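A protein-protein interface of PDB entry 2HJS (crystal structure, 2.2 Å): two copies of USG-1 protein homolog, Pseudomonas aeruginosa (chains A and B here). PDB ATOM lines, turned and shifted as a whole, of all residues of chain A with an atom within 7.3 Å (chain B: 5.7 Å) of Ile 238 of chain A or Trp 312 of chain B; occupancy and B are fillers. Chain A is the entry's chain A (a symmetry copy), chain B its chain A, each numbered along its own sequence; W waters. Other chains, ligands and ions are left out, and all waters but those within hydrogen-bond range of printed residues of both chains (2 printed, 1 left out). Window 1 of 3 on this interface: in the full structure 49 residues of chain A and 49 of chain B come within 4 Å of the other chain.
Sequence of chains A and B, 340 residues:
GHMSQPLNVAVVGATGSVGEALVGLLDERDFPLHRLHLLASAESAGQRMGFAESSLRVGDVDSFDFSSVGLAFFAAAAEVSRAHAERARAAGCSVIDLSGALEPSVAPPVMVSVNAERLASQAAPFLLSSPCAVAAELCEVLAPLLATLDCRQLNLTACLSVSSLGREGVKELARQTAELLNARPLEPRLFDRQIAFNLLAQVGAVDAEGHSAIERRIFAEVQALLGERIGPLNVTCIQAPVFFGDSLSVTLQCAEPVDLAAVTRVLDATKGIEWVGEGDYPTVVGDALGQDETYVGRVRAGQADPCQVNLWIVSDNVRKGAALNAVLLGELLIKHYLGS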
ATOM      1  N   THR A 157     -22.149 -15.555  18.934  1.00  0.00           N
ATOM      2  CA  THR A 157     -20.817 -15.962  18.501  1.00  0.00           C
ATOM      3  C   THR A 157     -20.564 -17.333  19.124  1.00  0.00           C
ATOM      4  O   THR A 157     -20.429 -17.454  20.335  1.00  0.00           O
ATOM      5  CB  THR A 157     -19.721 -14.990  18.962  1.00  0.00           C
ATOM      6  OG1 THR A 157     -20.003 -13.681  18.457  1.00  0.00           O
ATOM      7  CG2 THR A 157     -18.346 -15.438  18.453  1.00  0.00           C
ATOM      8  N   ALA A 158     -20.494 -18.363  18.296  1.00  0.00           N
ATOM      9  CA  ALA A 158     -20.322 -19.708  18.799  1.00  0.00           C
ATOM     10  C   ALA A 158     -18.891 -20.159  18.592  1.00  0.00           C
ATOM     11  O   ALA A 158     -18.400 -20.132  17.466  1.00  0.00           O
ATOM     12  CB  ALA A 158     -21.288 -20.659  18.083  1.00  0.00           C
ATOM     13  N   CYS A 159     -18.215 -20.543  19.667  1.00  0.00           N
ATOM     14  CA  CYS A 159     -16.853 -21.081  19.579  1.00  0.00           C
ATOM     15  C   CYS A 159     -16.925 -22.586  19.672  1.00  0.00           C
ATOM     16  O   CYS A 159     -17.243 -23.147  20.736  1.00  0.00           O
ATOM     17  CB  CYS A 159     -15.975 -20.520  20.682  1.00  0.00           C
ATOM     18  SG  CYS A 159     -15.855 -18.699  20.579  1.00  0.00           S
ATOM     19  N   LEU A 160     -16.668 -23.235  18.541  1.00  0.00           N
ATOM     20  CA  LEU A 160     -16.890 -24.663  18.395  1.00  0.00           C
ATOM     21  C   LEU A 160     -15.585 -25.404  18.675  1.00  0.00           C
ATOM     22  O   LEU A 160     -14.523 -24.966  18.245  1.00  0.00           O
ATOM     23  CB  LEU A 160     -17.372 -24.977  16.966  1.00  0.00           C
ATOM     24  CG  LEU A 160     -18.883 -24.961  16.682  1.00  0.00           C
ATOM     25  CD1 LEU A 160     -19.520 -23.689  17.051  1.00  0.00           C
ATOM     26  CD2 LEU A 160     -19.196 -25.274  15.194  1.00  0.00           C
ATOM     27  N   SER A 161     -15.679 -26.517  19.388  1.00  0.00           N
ATOM     28  CA  SER A 161     -14.538 -27.423  19.578  1.00  0.00           C
ATOM     29  C   SER A 161     -14.326 -28.272  18.322  1.00  0.00           C
ATOM     30  O   SER A 161     -15.230 -28.372  17.483  1.00  0.00           O
ATOM     31  CB  SER A 161     -14.845 -28.361  20.734  1.00  0.00           C
ATOM     32  OG  SER A 161     -15.884 -29.260  20.377  1.00  0.00           O
ATOM     33  N   ASN A 198      -4.858 -21.928  17.373  1.00  0.00           N
ATOM     34  CA  ASN A 198      -5.329 -20.971  16.363  1.00  0.00           C
ATOM     35  C   ASN A 198      -6.835 -20.836  16.445  1.00  0.00           C
ATOM     36  O   ASN A 198      -7.493 -21.734  16.935  1.00  0.00           O
ATOM     37  CB  ASN A 198      -4.929 -21.433  14.957  1.00  0.00           C
ATOM     38  CG  ASN A 198      -4.712 -20.269  14.000  1.00  0.00           C
ATOM     39  OD1 ASN A 198      -4.731 -19.117  14.414  1.00  0.00           O
ATOM     40  ND2 ASN A 198      -4.464 -20.568  12.728  1.00  0.00           N
ATOM     41  N   LEU A 199      -7.384 -19.709  15.998  1.00  0.00           N
ATOM     42  CA  LEU A 199      -8.848 -19.557  15.911  1.00  0.00           C
ATOM     43  C   LEU A 199      -9.218 -19.393  14.450  1.00  0.00           C
ATOM     44  O   LEU A 199      -8.697 -18.487  13.782  1.00  0.00           O
ATOM     45  CB  LEU A 199      -9.348 -18.362  16.750  1.00  0.00           C
ATOM     46  CG  LEU A 199      -9.309 -18.574  18.274  1.00  0.00           C
ATOM     47  CD1 LEU A 199      -9.242 -17.236  18.985  1.00  0.00           C
ATOM     48  CD2 LEU A 199     -10.471 -19.398  18.806  1.00  0.00           C
ATOM     49  N   LEU A 200     -10.055 -20.286  13.927  1.00  0.00           N
ATOM     50  CA  LEU A 200     -10.469 -20.156  12.528  1.00  0.00           C
ATOM     51  C   LEU A 200     -11.724 -19.301  12.455  1.00  0.00           C
ATOM     52  O   LEU A 200     -12.627 -19.457  13.267  1.00  0.00           O
ATOM     53  CB  LEU A 200     -10.700 -21.520  11.865  1.00  0.00           C
ATOM     54  CG  LEU A 200      -9.654 -22.620  12.096  1.00  0.00           C
ATOM     55  CD1 LEU A 200     -10.002 -23.837  11.221  1.00  0.00           C
ATOM     56  CD2 LEU A 200      -8.238 -22.107  11.809  1.00  0.00           C
ATOM     57  N   ALA A 201     -11.786 -18.410  11.469  1.00  0.00           N
ATOM     58  CA  ALA A 201     -12.911 -17.476  11.360  1.00  0.00           C
ATOM     59  C   ALA A 201     -14.249 -18.137  11.043  1.00  0.00           C
ATOM     60  O   ALA A 201     -15.301 -17.563  11.326  1.00  0.00           O
ATOM     61  CB  ALA A 201     -12.588 -16.394  10.306  1.00  0.00           C
ATOM     62  N   GLN A 202     -14.203 -19.318  10.426  1.00  0.00           N
ATOM     63  CA  GLN A 202     -15.384 -20.020   9.955  1.00  0.00           C
ATOM     64  C   GLN A 202     -15.153 -21.511  10.104  1.00  0.00           C
ATOM     65  O   GLN A 202     -13.995 -21.961  10.182  1.00  0.00           O
ATOM     66  CB  GLN A 202     -15.670 -19.707   8.467  1.00  0.00           C
ATOM     67  CG  GLN A 202     -14.632 -20.231   7.509  1.00  0.00           C
ATOM     68  CD  GLN A 202     -14.528 -19.387   6.241  1.00  0.00           C
ATOM     69  OE1 GLN A 202     -14.656 -18.161   6.279  1.00  0.00           O
ATOM     70  NE2 GLN A 202     -14.323 -20.041   5.115  1.00  0.00           N
ATOM     71  N   VAL A 203     -16.251 -22.270  10.126  1.00  0.00           N
ATOM     72  CA  VAL A 203     -16.189 -23.742  10.126  1.00  0.00           C
ATOM     73  C   VAL A 203     -16.610 -24.265   8.718  1.00  0.00           C
ATOM     74  O   VAL A 203     -17.781 -24.263   8.368  1.00  0.00           O
ATOM     75  CB  VAL A 203     -17.072 -24.310  11.261  1.00  0.00           C
ATOM     76  CG1 VAL A 203     -17.124 -25.838  11.239  1.00  0.00           C
ATOM     77  CG2 VAL A 203     -16.600 -23.801  12.629  1.00  0.00           C
ATOM     78  N   ILE A 214     -22.811 -24.715   8.821  1.00  0.00           N
ATOM     79  CA  ILE A 214     -23.294 -24.795  10.205  1.00  0.00           C
ATOM     80  C   ILE A 214     -24.072 -23.524  10.600  1.00  0.00           C
ATOM     81  O   ILE A 214     -25.062 -23.602  11.298  1.00  0.00           O
ATOM     82  CB  ILE A 214     -22.151 -25.170  11.225  1.00  0.00           C
ATOM     83  CG1 ILE A 214     -22.731 -25.438  12.619  1.00  0.00           C
ATOM     84  CG2 ILE A 214     -21.098 -24.074  11.335  1.00  0.00           C
ATOM     85  CD1 ILE A 214     -23.741 -26.560  12.658  1.00  0.00           C
ATOM     86  N   GLU A 215     -23.634 -22.374  10.115  1.00  0.00           N
ATOM     87  CA  GLU A 215     -24.307 -21.089  10.358  1.00  0.00           C
ATOM     88  C   GLU A 215     -25.726 -21.038   9.742  1.00  0.00           C
ATOM     89  O   GLU A 215     -26.671 -20.543  10.376  1.00  0.00           O
ATOM     90  CB  GLU A 215     -23.448 -19.955   9.810  1.00  0.00           C
ATOM     91  CG  GLU A 215     -22.305 -19.600  10.730  1.00  0.00           C
ATOM     92  CD  GLU A 215     -21.212 -18.758  10.076  1.00  0.00           C
ATOM     93  OE1 GLU A 215     -21.380 -18.274   8.912  1.00  0.00           O
ATOM     94  OE2 GLU A 215     -20.160 -18.575  10.740  1.00  0.00           O
ATOM     95  N   THR A 236     -22.228 -16.286  14.078  1.00  0.00           N
ATOM     96  CA  THR A 236     -20.876 -16.552  13.660  1.00  0.00           C
ATOM     97  C   THR A 236     -20.402 -17.813  14.375  1.00  0.00           C
ATOM     98  O   THR A 236     -20.463 -17.898  15.607  1.00  0.00           O
ATOM     99  CB  THR A 236     -19.955 -15.377  14.026  1.00  0.00           C
ATOM    100  OG1 THR A 236     -20.520 -14.175  13.485  1.00  0.00           O
ATOM    101  CG2 THR A 236     -18.555 -15.575  13.449  1.00  0.00           C
ATOM    102  N   CYS A 237     -19.944 -18.797  13.606  1.00  0.00           N
ATOM    103  CA  CYS A 237     -19.301 -19.966  14.204  1.00  0.00           C
ATOM    104  C   CYS A 237     -17.811 -19.961  13.934  1.00  0.00           C
ATOM    105  O   CYS A 237     -17.366 -19.978  12.782  1.00  0.00           O
ATOM    106  CB  CYS A 237     -19.924 -21.275  13.720  1.00  0.00           C
ATOM    107  SG  CYS A 237     -21.629 -21.427  14.256  1.00  0.00           S
ATOM    108  N   ILE A 238     -17.055 -19.975  15.017  1.00  0.00           N
ATOM    109  CA  ILE A 238     -15.608 -19.925  14.983  1.00  0.00           C
ATOM    110  C   ILE A 238     -15.111 -21.300  15.402  1.00  0.00           C
ATOM    111  O   ILE A 238     -15.752 -21.977  16.208  1.00  0.00           O
ATOM    112  CB  ILE A 238     -15.132 -18.848  15.988  1.00  0.00           C
ATOM    113  CG1 ILE A 238     -15.417 -17.471  15.420  1.00  0.00           C
ATOM    114  CG2 ILE A 238     -13.650 -18.969  16.355  1.00  0.00           C
ATOM    115  CD1 ILE A 238     -15.501 -16.459  16.571  1.00  0.00           C
ATOM    116  N   GLN A 239     -13.980 -21.717  14.847  1.00  0.00           N
ATOM    117  CA  GLN A 239     -13.367 -22.978  15.247  1.00  0.00           C
ATOM    118  C   GLN A 239     -12.263 -22.718  16.284  1.00  0.00           C
ATOM    119  O   GLN A 239     -11.272 -22.054  15.971  1.00  0.00           O
ATOM    120  CB  GLN A 239     -12.736 -23.644  14.032  1.00  0.00           C
ATOM    121  CG  GLN A 239     -12.157 -24.997  14.340  1.00  0.00           C
ATOM    122  CD  GLN A 239     -13.193 -26.036  14.211  1.00  0.00           C
ATOM    123  OE1 GLN A 239     -13.595 -26.385  13.094  1.00  0.00           O
ATOM    124  NE2 GLN A 239     -13.688 -26.530  15.350  1.00  0.00           N
ATOM    125  N   ALA A 240     -12.426 -23.237  17.503  1.00  0.00           N
ATOM    126  CA  ALA A 240     -11.437 -23.001  18.571  1.00  0.00           C
ATOM    127  C   ALA A 240     -10.533 -24.212  18.737  1.00  0.00           C
ATOM    128  O   ALA A 240     -10.954 -25.344  18.453  1.00  0.00           O
ATOM    129  CB  ALA A 240     -12.148 -22.681  19.902  1.00  0.00           C
ATOM    130  N   PRO A 241      -9.279 -23.995  19.197  1.00  0.00           N
ATOM    131  CA  PRO A 241      -8.453 -25.188  19.409  1.00  0.00           C
ATOM    132  C   PRO A 241      -8.811 -25.859  20.756  1.00  0.00           C
ATOM    133  O   PRO A 241      -8.024 -25.839  21.712  1.00  0.00           O
ATOM    134  CB  PRO A 241      -7.033 -24.626  19.402  1.00  0.00           C
ATOM    135  CG  PRO A 241      -7.202 -23.191  19.946  1.00  0.00           C
ATOM    136  CD  PRO A 241      -8.571 -22.743  19.545  1.00  0.00           C
ATOM    137  N   SER A 247     -18.979 -23.440  23.293  1.00  0.00           N
ATOM    138  CA  SER A 247     -18.943 -22.248  24.138  1.00  0.00           C
ATOM    139  C   SER A 247     -19.629 -21.089  23.388  1.00  0.00           C
ATOM    140  O   SER A 247     -19.156 -20.670  22.343  1.00  0.00           O
ATOM    141  CB  SER A 247     -17.489 -21.856  24.468  1.00  0.00           C
ATOM    142  OG  SER A 247     -16.794 -22.950  25.061  1.00  0.00           O
ATOM    143  N   CYS B 159     -11.783 -12.617  21.144  1.00  0.00           N
ATOM    144  CA  CYS B 159     -11.091 -13.820  21.621  1.00  0.00           C
ATOM    145  C   CYS B 159      -9.626 -13.494  21.793  1.00  0.00           C
ATOM    146  O   CYS B 159      -8.899 -13.280  20.806  1.00  0.00           O
ATOM    147  CB  CYS B 159     -11.270 -14.972  20.650  1.00  0.00           C
ATOM    148  SG  CYS B 159     -13.035 -15.400  20.441  1.00  0.00           S
ATOM    149  N   SER B 247      -8.307 -12.018  18.032  1.00  0.00           N
ATOM    150  CA  SER B 247      -9.270 -12.424  17.010  1.00  0.00           C
ATOM    151  C   SER B 247     -10.649 -11.834  17.369  1.00  0.00           C
ATOM    152  O   SER B 247     -11.214 -12.176  18.398  1.00  0.00           O
ATOM    153  CB  SER B 247      -9.373 -13.960  16.938  1.00  0.00           C
ATOM    154  OG  SER B 247      -8.090 -14.541  16.720  1.00  0.00           O
ATOM    155  N   LEU B 248     -11.184 -10.949  16.534  1.00  0.00           N
ATOM    156  CA  LEU B 248     -12.403 -10.228  16.890  1.00  0.00           C
ATOM    157  C   LEU B 248     -13.550 -10.579  15.951  1.00  0.00           C
ATOM    158  O   LEU B 248     -13.369 -10.577  14.741  1.00  0.00           O
ATOM    159  CB  LEU B 248     -12.180  -8.708  16.831  1.00  0.00           C
ATOM    160  CG  LEU B 248     -10.906  -8.122  17.472  1.00  0.00           C
ATOM    161  CD1 LEU B 248     -10.915  -6.599  17.337  1.00  0.00           C
ATOM    162  CD2 LEU B 248     -10.814  -8.532  18.944  1.00  0.00           C
ATOM    163  N   SER B 249     -14.719 -10.862  16.517  1.00  0.00           N
ATOM    164  CA  SER B 249     -15.923 -11.031  15.727  1.00  0.00           C
ATOM    165  C   SER B 249     -16.860  -9.861  16.017  1.00  0.00           C
ATOM    166  O   SER B 249     -17.306  -9.655  17.140  1.00  0.00           O
ATOM    167  CB  SER B 249     -16.585 -12.373  16.033  1.00  0.00           C
ATOM    168  OG  SER B 249     -17.808 -12.453  15.329  1.00  0.00           O
ATOM    169  N   VAL B 250     -17.124  -9.076  14.978  1.00  0.00           N
ATOM    170  CA  VAL B 250     -17.850  -7.818  15.095  1.00  0.00           C
ATOM    171  C   VAL B 250     -19.162  -7.911  14.318  1.00  0.00           C
ATOM    172  O   VAL B 250     -19.185  -8.466  13.227  1.00  0.00           O
ATOM    173  CB  VAL B 250     -16.964  -6.657  14.549  1.00  0.00           C
ATOM    174  CG1 VAL B 250     -17.683  -5.299  14.628  1.00  0.00           C
ATOM    175  CG2 VAL B 250     -15.589  -6.587  15.307  1.00  0.00           C
ATOM    176  N   TYR B 281     -10.006 -16.547   4.798  1.00  0.00           N
ATOM    177  CA  TYR B 281     -10.016 -15.756   6.021  1.00  0.00           C
ATOM    178  C   TYR B 281      -8.605 -15.697   6.616  1.00  0.00           C
ATOM    179  O   TYR B 281      -7.824 -16.622   6.450  1.00  0.00           O
ATOM    180  CB  TYR B 281     -11.043 -16.322   7.039  1.00  0.00           C
ATOM    181  CG  TYR B 281     -10.745 -17.756   7.448  1.00  0.00           C
ATOM    182  CD1 TYR B 281      -9.901 -18.043   8.534  1.00  0.00           C
ATOM    183  CD2 TYR B 281     -11.279 -18.828   6.721  1.00  0.00           C
ATOM    184  CE1 TYR B 281      -9.595 -19.357   8.875  1.00  0.00           C
ATOM    185  CE2 TYR B 281     -10.979 -20.129   7.047  1.00  0.00           C
ATOM    186  CZ  TYR B 281     -10.147 -20.396   8.129  1.00  0.00           C
ATOM    187  OH  TYR B 281      -9.871 -21.709   8.428  1.00  0.00           O
ATOM    188  N   PRO B 282      -8.279 -14.605   7.324  1.00  0.00           N
ATOM    189  CA  PRO B 282      -7.021 -14.579   8.051  1.00  0.00           C
ATOM    190  C   PRO B 282      -7.124 -15.205   9.445  1.00  0.00           C
ATOM    191  O   PRO B 282      -8.236 -15.282  10.039  1.00  0.00           O
ATOM    192  CB  PRO B 282      -6.742 -13.092   8.176  1.00  0.00           C
ATOM    193  CG  PRO B 282      -8.136 -12.493   8.358  1.00  0.00           C
ATOM    194  CD  PRO B 282      -9.041 -13.346   7.469  1.00  0.00           C
ATOM    195  N   THR B 283      -5.980 -15.633   9.977  1.00  0.00           N
ATOM    196  CA  THR B 283      -5.924 -16.097  11.383  1.00  0.00           C
ATOM    197  C   THR B 283      -4.738 -15.449  12.099  1.00  0.00           C
ATOM    198  O   THR B 283      -3.829 -14.932  11.436  1.00  0.00           O
ATOM    199  CB  THR B 283      -5.779 -17.638  11.508  1.00  0.00           C
ATOM    200  OG1 THR B 283      -4.501 -18.031  10.979  1.00  0.00           O
ATOM    201  CG2 THR B 283      -6.907 -18.368  10.793  1.00  0.00           C
ATOM    202  N   TYR B 295      -5.670  -7.569   9.747  1.00  0.00           N
ATOM    203  CA  TYR B 295      -6.368  -8.320   8.695  1.00  0.00           C
ATOM    204  C   TYR B 295      -7.869  -8.359   8.962  1.00  0.00           C
ATOM    205  O   TYR B 295      -8.279  -8.565  10.091  1.00  0.00           O
ATOM    206  CB  TYR B 295      -5.851  -9.742   8.662  1.00  0.00           C
ATOM    207  CG  TYR B 295      -4.518  -9.907   7.999  1.00  0.00           C
ATOM    208  CD1 TYR B 295      -4.440 -10.395   6.701  1.00  0.00           C
ATOM    209  CD2 TYR B 295      -3.324  -9.573   8.660  1.00  0.00           C
ATOM    210  CE1 TYR B 295      -3.214 -10.571   6.066  1.00  0.00           C
ATOM    211  CE2 TYR B 295      -2.083  -9.734   8.024  1.00  0.00           C
ATOM    212  CZ  TYR B 295      -2.050 -10.231   6.727  1.00  0.00           C
ATOM    213  OH  TYR B 295      -0.857 -10.414   6.071  1.00  0.00           O
ATOM    214  N   VAL B 296      -8.681  -8.154   7.925  1.00  0.00           N
ATOM    215  CA  VAL B 296     -10.125  -8.124   8.088  1.00  0.00           C
ATOM    216  C   VAL B 296     -10.742  -9.033   7.032  1.00  0.00           C
ATOM    217  O   VAL B 296     -10.449  -8.871   5.855  1.00  0.00           O
ATOM    218  CB  VAL B 296     -10.715  -6.692   7.918  1.00  0.00           C
ATOM    219  CG1 VAL B 296     -12.252  -6.690   8.206  1.00  0.00           C
ATOM    220  CG2 VAL B 296     -10.023  -5.730   8.838  1.00  0.00           C
ATOM    221  N   GLY B 297     -11.596  -9.968   7.461  1.00  0.00           N
ATOM    222  CA  GLY B 297     -12.326 -10.836   6.553  1.00  0.00           C
ATOM    223  C   GLY B 297     -13.768 -11.120   6.948  1.00  0.00           C
ATOM    224  O   GLY B 297     -14.299 -10.522   7.897  1.00  0.00           O
ATOM    225  N   ARG B 298     -14.392 -12.031   6.193  1.00  0.00           N
ATOM    226  CA  ARG B 298     -15.747 -12.529   6.409  1.00  0.00           C
ATOM    227  C   ARG B 298     -16.771 -11.408   6.374  1.00  0.00           C
ATOM    228  O   ARG B 298     -17.750 -11.441   7.113  1.00  0.00           O
ATOM    229  CB  ARG B 298     -15.870 -13.367   7.706  1.00  0.00           C
ATOM    230  CG  ARG B 298     -15.010 -14.628   7.760  1.00  0.00           C
ATOM    231  CD  ARG B 298     -15.700 -15.715   8.556  1.00  0.00           C
ATOM    232  NE  ARG B 298     -16.997 -16.057   7.966  1.00  0.00           N
ATOM    233  CZ  ARG B 298     -18.004 -16.647   8.590  1.00  0.00           C
ATOM    234  NH1 ARG B 298     -17.878 -17.027   9.858  1.00  0.00           N
ATOM    235  NH2 ARG B 298     -19.142 -16.889   7.921  1.00  0.00           N
ATOM    236  N   VAL B 299     -16.523 -10.405   5.532  1.00  0.00           N
ATOM    237  CA  VAL B 299     -17.457  -9.291   5.379  1.00  0.00           C
ATOM    238  C   VAL B 299     -18.707  -9.834   4.714  1.00  0.00           C
ATOM    239  O   VAL B 299     -18.643 -10.332   3.606  1.00  0.00           O
ATOM    240  CB  VAL B 299     -16.854  -8.133   4.542  1.00  0.00           C
ATOM    241  CG1 VAL B 299     -17.940  -7.046   4.231  1.00  0.00           C
ATOM    242  CG2 VAL B 299     -15.658  -7.524   5.254  1.00  0.00           C
ATOM    243  N   ASN B 310     -21.176  -8.173   9.287  1.00  0.00           N
ATOM    244  CA  ASN B 310     -20.200  -8.817  10.156  1.00  0.00           C
ATOM    245  C   ASN B 310     -18.813  -8.585   9.634  1.00  0.00           C
ATOM    246  O   ASN B 310     -18.638  -8.484   8.432  1.00  0.00           O
ATOM    247  CB  ASN B 310     -20.419 -10.319  10.166  1.00  0.00           C
ATOM    248  CG  ASN B 310     -21.681 -10.704  10.874  1.00  0.00           C
ATOM    249  OD1 ASN B 310     -22.746 -10.809  10.259  1.00  0.00           O
ATOM    250  ND2 ASN B 310     -21.592 -10.856  12.192  1.00  0.00           N
ATOM    251  N   LEU B 311     -17.841  -8.501  10.548  1.00  0.00           N
ATOM    252  CA  LEU B 311     -16.432  -8.420  10.194  1.00  0.00           C
ATOM    253  C   LEU B 311     -15.692  -9.386  11.112  1.00  0.00           C
ATOM    254  O   LEU B 311     -16.087  -9.563  12.249  1.00  0.00           O
ATOM    255  CB  LEU B 311     -15.856  -7.014  10.486  1.00  0.00           C
ATOM    256  CG  LEU B 311     -16.567  -5.746  10.018  1.00  0.00           C
ATOM    257  CD1 LEU B 311     -15.906  -4.592  10.726  1.00  0.00           C
ATOM    258  CD2 LEU B 311     -16.379  -5.583   8.526  1.00  0.00           C
ATOM    259  N   TRP B 312     -14.585  -9.942  10.625  1.00  0.00           N
ATOM    260  CA  TRP B 312     -13.665 -10.720  11.448  1.00  0.00           C
ATOM    261  C   TRP B 312     -12.316 -10.038  11.340  1.00  0.00           C
ATOM    262  O   TRP B 312     -11.866  -9.736  10.253  1.00  0.00           O
ATOM    263  CB  TRP B 312     -13.614 -12.156  10.942  1.00  0.00           C
ATOM    264  CG  TRP B 312     -12.437 -13.014  11.401  1.00  0.00           C
ATOM    265  CD1 TRP B 312     -11.260 -13.244  10.705  1.00  0.00           C
ATOM    266  CD2 TRP B 312     -12.343 -13.794  12.610  1.00  0.00           C
ATOM    267  NE1 TRP B 312     -10.461 -14.109  11.422  1.00  0.00           N
ATOM    268  CE2 TRP B 312     -11.094 -14.455  12.588  1.00  0.00           C
ATOM    269  CE3 TRP B 312     -13.189 -13.986  13.715  1.00  0.00           C
ATOM    270  CZ2 TRP B 312     -10.685 -15.329  13.609  1.00  0.00           C
ATOM    271  CZ3 TRP B 312     -12.773 -14.843  14.739  1.00  0.00           C
ATOM    272  CH2 TRP B 312     -11.530 -15.511  14.665  1.00  0.00           C
ATOM    273  N   ILE B 313     -11.704  -9.739  12.481  1.00  0.00           N
ATOM    274  CA  ILE B 313     -10.488  -8.935  12.517  1.00  0.00           C
ATOM    275  C   ILE B 313      -9.400  -9.722  13.247  1.00  0.00           C
ATOM    276  O   ILE B 313      -9.648 -10.283  14.312  1.00  0.00           O
ATOM    277  CB  ILE B 313     -10.734  -7.594  13.266  1.00  0.00           C
ATOM    278  CG1 ILE B 313     -11.914  -6.827  12.648  1.00  0.00           C
ATOM    279  CG2 ILE B 313      -9.431  -6.754  13.302  1.00  0.00           C
ATOM    280  CD1 ILE B 313     -12.369  -5.618  13.484  1.00  0.00           C
ATOM    281  N   VAL B 314      -8.208  -9.809  12.666  1.00  0.00           N
ATOM    282  CA  VAL B 314      -7.098 -10.394  13.415  1.00  0.00           C
ATOM    283  C   VAL B 314      -5.909  -9.473  13.347  1.00  0.00           C
ATOM    284  O   VAL B 314      -5.624  -8.873  12.308  1.00  0.00           O
ATOM    285  CB  VAL B 314      -6.730 -11.883  13.009  1.00  0.00           C
ATOM    286  CG1 VAL B 314      -7.926 -12.892  13.307  1.00  0.00           C
ATOM    287  CG2 VAL B 314      -6.236 -12.000  11.588  1.00  0.00           C
HETATM  288  O   HOH W   1     -18.540 -11.498  12.970  1.00  0.00           O
HETATM  289  O   HOH W   2      -7.322 -16.203  14.472  1.00  0.00           O
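The side-chain hydroxyl (OG1) of Thr 283 of chain B is in hydrogen-bond range of the side-chain amide nitrogen (ND2) of Asn 198 of chain A, at 3.1 Å. The guanidinium group (NH1) of Arg 298 of chain B is in hydrogen-bond range of the backbone carbonyl oxygen (O) of Ala 201 of chain A. The side-chain carboxylate (OE1) of Glu 215 of chain A is in salt-bridge range of the guanidinium group (NH2) of Arg 298 of chain B, 2.8 Å away.
The backbone carbonyl oxygen of Ser 247 of chain B sits at hydrogen-bond distance from the backbone NH of Cys 159 of chain B (2.8 Å). O of Gly 297 of chain B lies within hydrogen-bond range of N of Trp 312 of chain B (2.8 Å). O of Thr 236 of chain A lies within hydrogen-bond range of N of Ala 158 of chain A (2.7 Å). O of Ala 158 of chain A sits at hydrogen-bond distance from N of Ile 238 of chain A, at 2.8 Å. O of Ile 238 of chain A is in hydrogen-bond range of N of Leu 160 of chain A. The backbone NH (N) of Leu 200 of chain A lies within hydrogen-bond range of the backbone carbonyl oxygen (O) of Gln 239 of chain A.
CG2 of Thr 283 of chain B touches O of Leu 199 of chain A, 3.5 Å away. Trp 312 of chain B touches Leu 199 of chain A (CZ2 to O, 3.7 Å). Leu 200 of chain A touches Tyr 281 of chain B. Tyr 281 of chain B touches Ala 201 of chain A (CD1 to N, 3.5 Å). CB of Ala 201 of chain A touches NE1 of Trp 312 of chain B (3.3 Å). Tyr 281 of chain B touches Gln 202 of chain A. OG of Ser 249 of chain B touches OG1 of Thr 236 of chain A, at 3.7 Å. Arg 298 of chain B touches Thr 236 of chain A. Asn 310 of chain B touches Thr 236 of chain A. Ile 238 of chain A touches Trp 312 of chain B (CD1 to CZ3, 3.7 Å).
Thr 157 of chain A touches none of the printed residues of chain B. Printed residues of chain B within 4 Å of Asn 198 of chain A: Thr 283 (3.1 Å). Ile 214 of chain A touches none of the printed residues of chain B. Printed residues of chain B within 4 Å of Glu 215 of chain A: Arg 298. Ile 238 of chain A touches just one residue of chain B: Trp 312. Of the printed residues of chain A, Ser 247 of chain B touches Leu 199. Of the printed residues of chain A, Tyr 281 of chain B touches Leu 200 (3.5 Å), Ala 201 (3.5 Å) and Gln 202 (3.3 Å). Of the printed residues of chain A, Arg 298 of chain B touches Ala 201 (3.0 Å), Gln 202 (3.5 Å), Glu 215 (2.8 Å) and Thr 236 (3.9 Å). Of chain A, only Leu 199, Ala 201 and Ile 238 come within 4 Å of Trp 312 of chain B. The nearest printed residue of chain B that does not touch Glu 215 of chain A is Asn 310 of chain B (7.7 Å).
Of the 18 printed residues of chain B, 8 touch a printed residue of chain A. Among the printed residues, 16 pairs touch across the chains. Among the printed residues, Asp or Glu carboxylates within 4 Å of a Lys or Arg side-chain nitrogen of the other chain: Glu 215 of chain A with Arg 298 of chain B (2.8 Å).
2 positions are printed for both chains. Of the 16 pairs that touch across the chains among the printed residues, none has its exchanged pair printed and touching as well.
Water W1 lies within hydrogen-bond range of the side-chain hydroxyl (OG) of Ser 249 of chain B (2.6 Å), the backbone carbonyl oxygen (O) of Val 250 of chain B (3.1 Å), the backbone carbonyl oxygen (O) of Leu 311 of chain B (3.2 Å), the side-chain amide nitrogen (ND2) of Asn 310 of chain B (3.2 Å) and the side-chain hydroxyl (OG1) of Thr 236 of chain A (3.4 Å). Water W2 lies within hydrogen-bond range of O of Leu 199 of chain A (2.8 Å) and OG of Ser 247 of chain B (2.9 Å).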
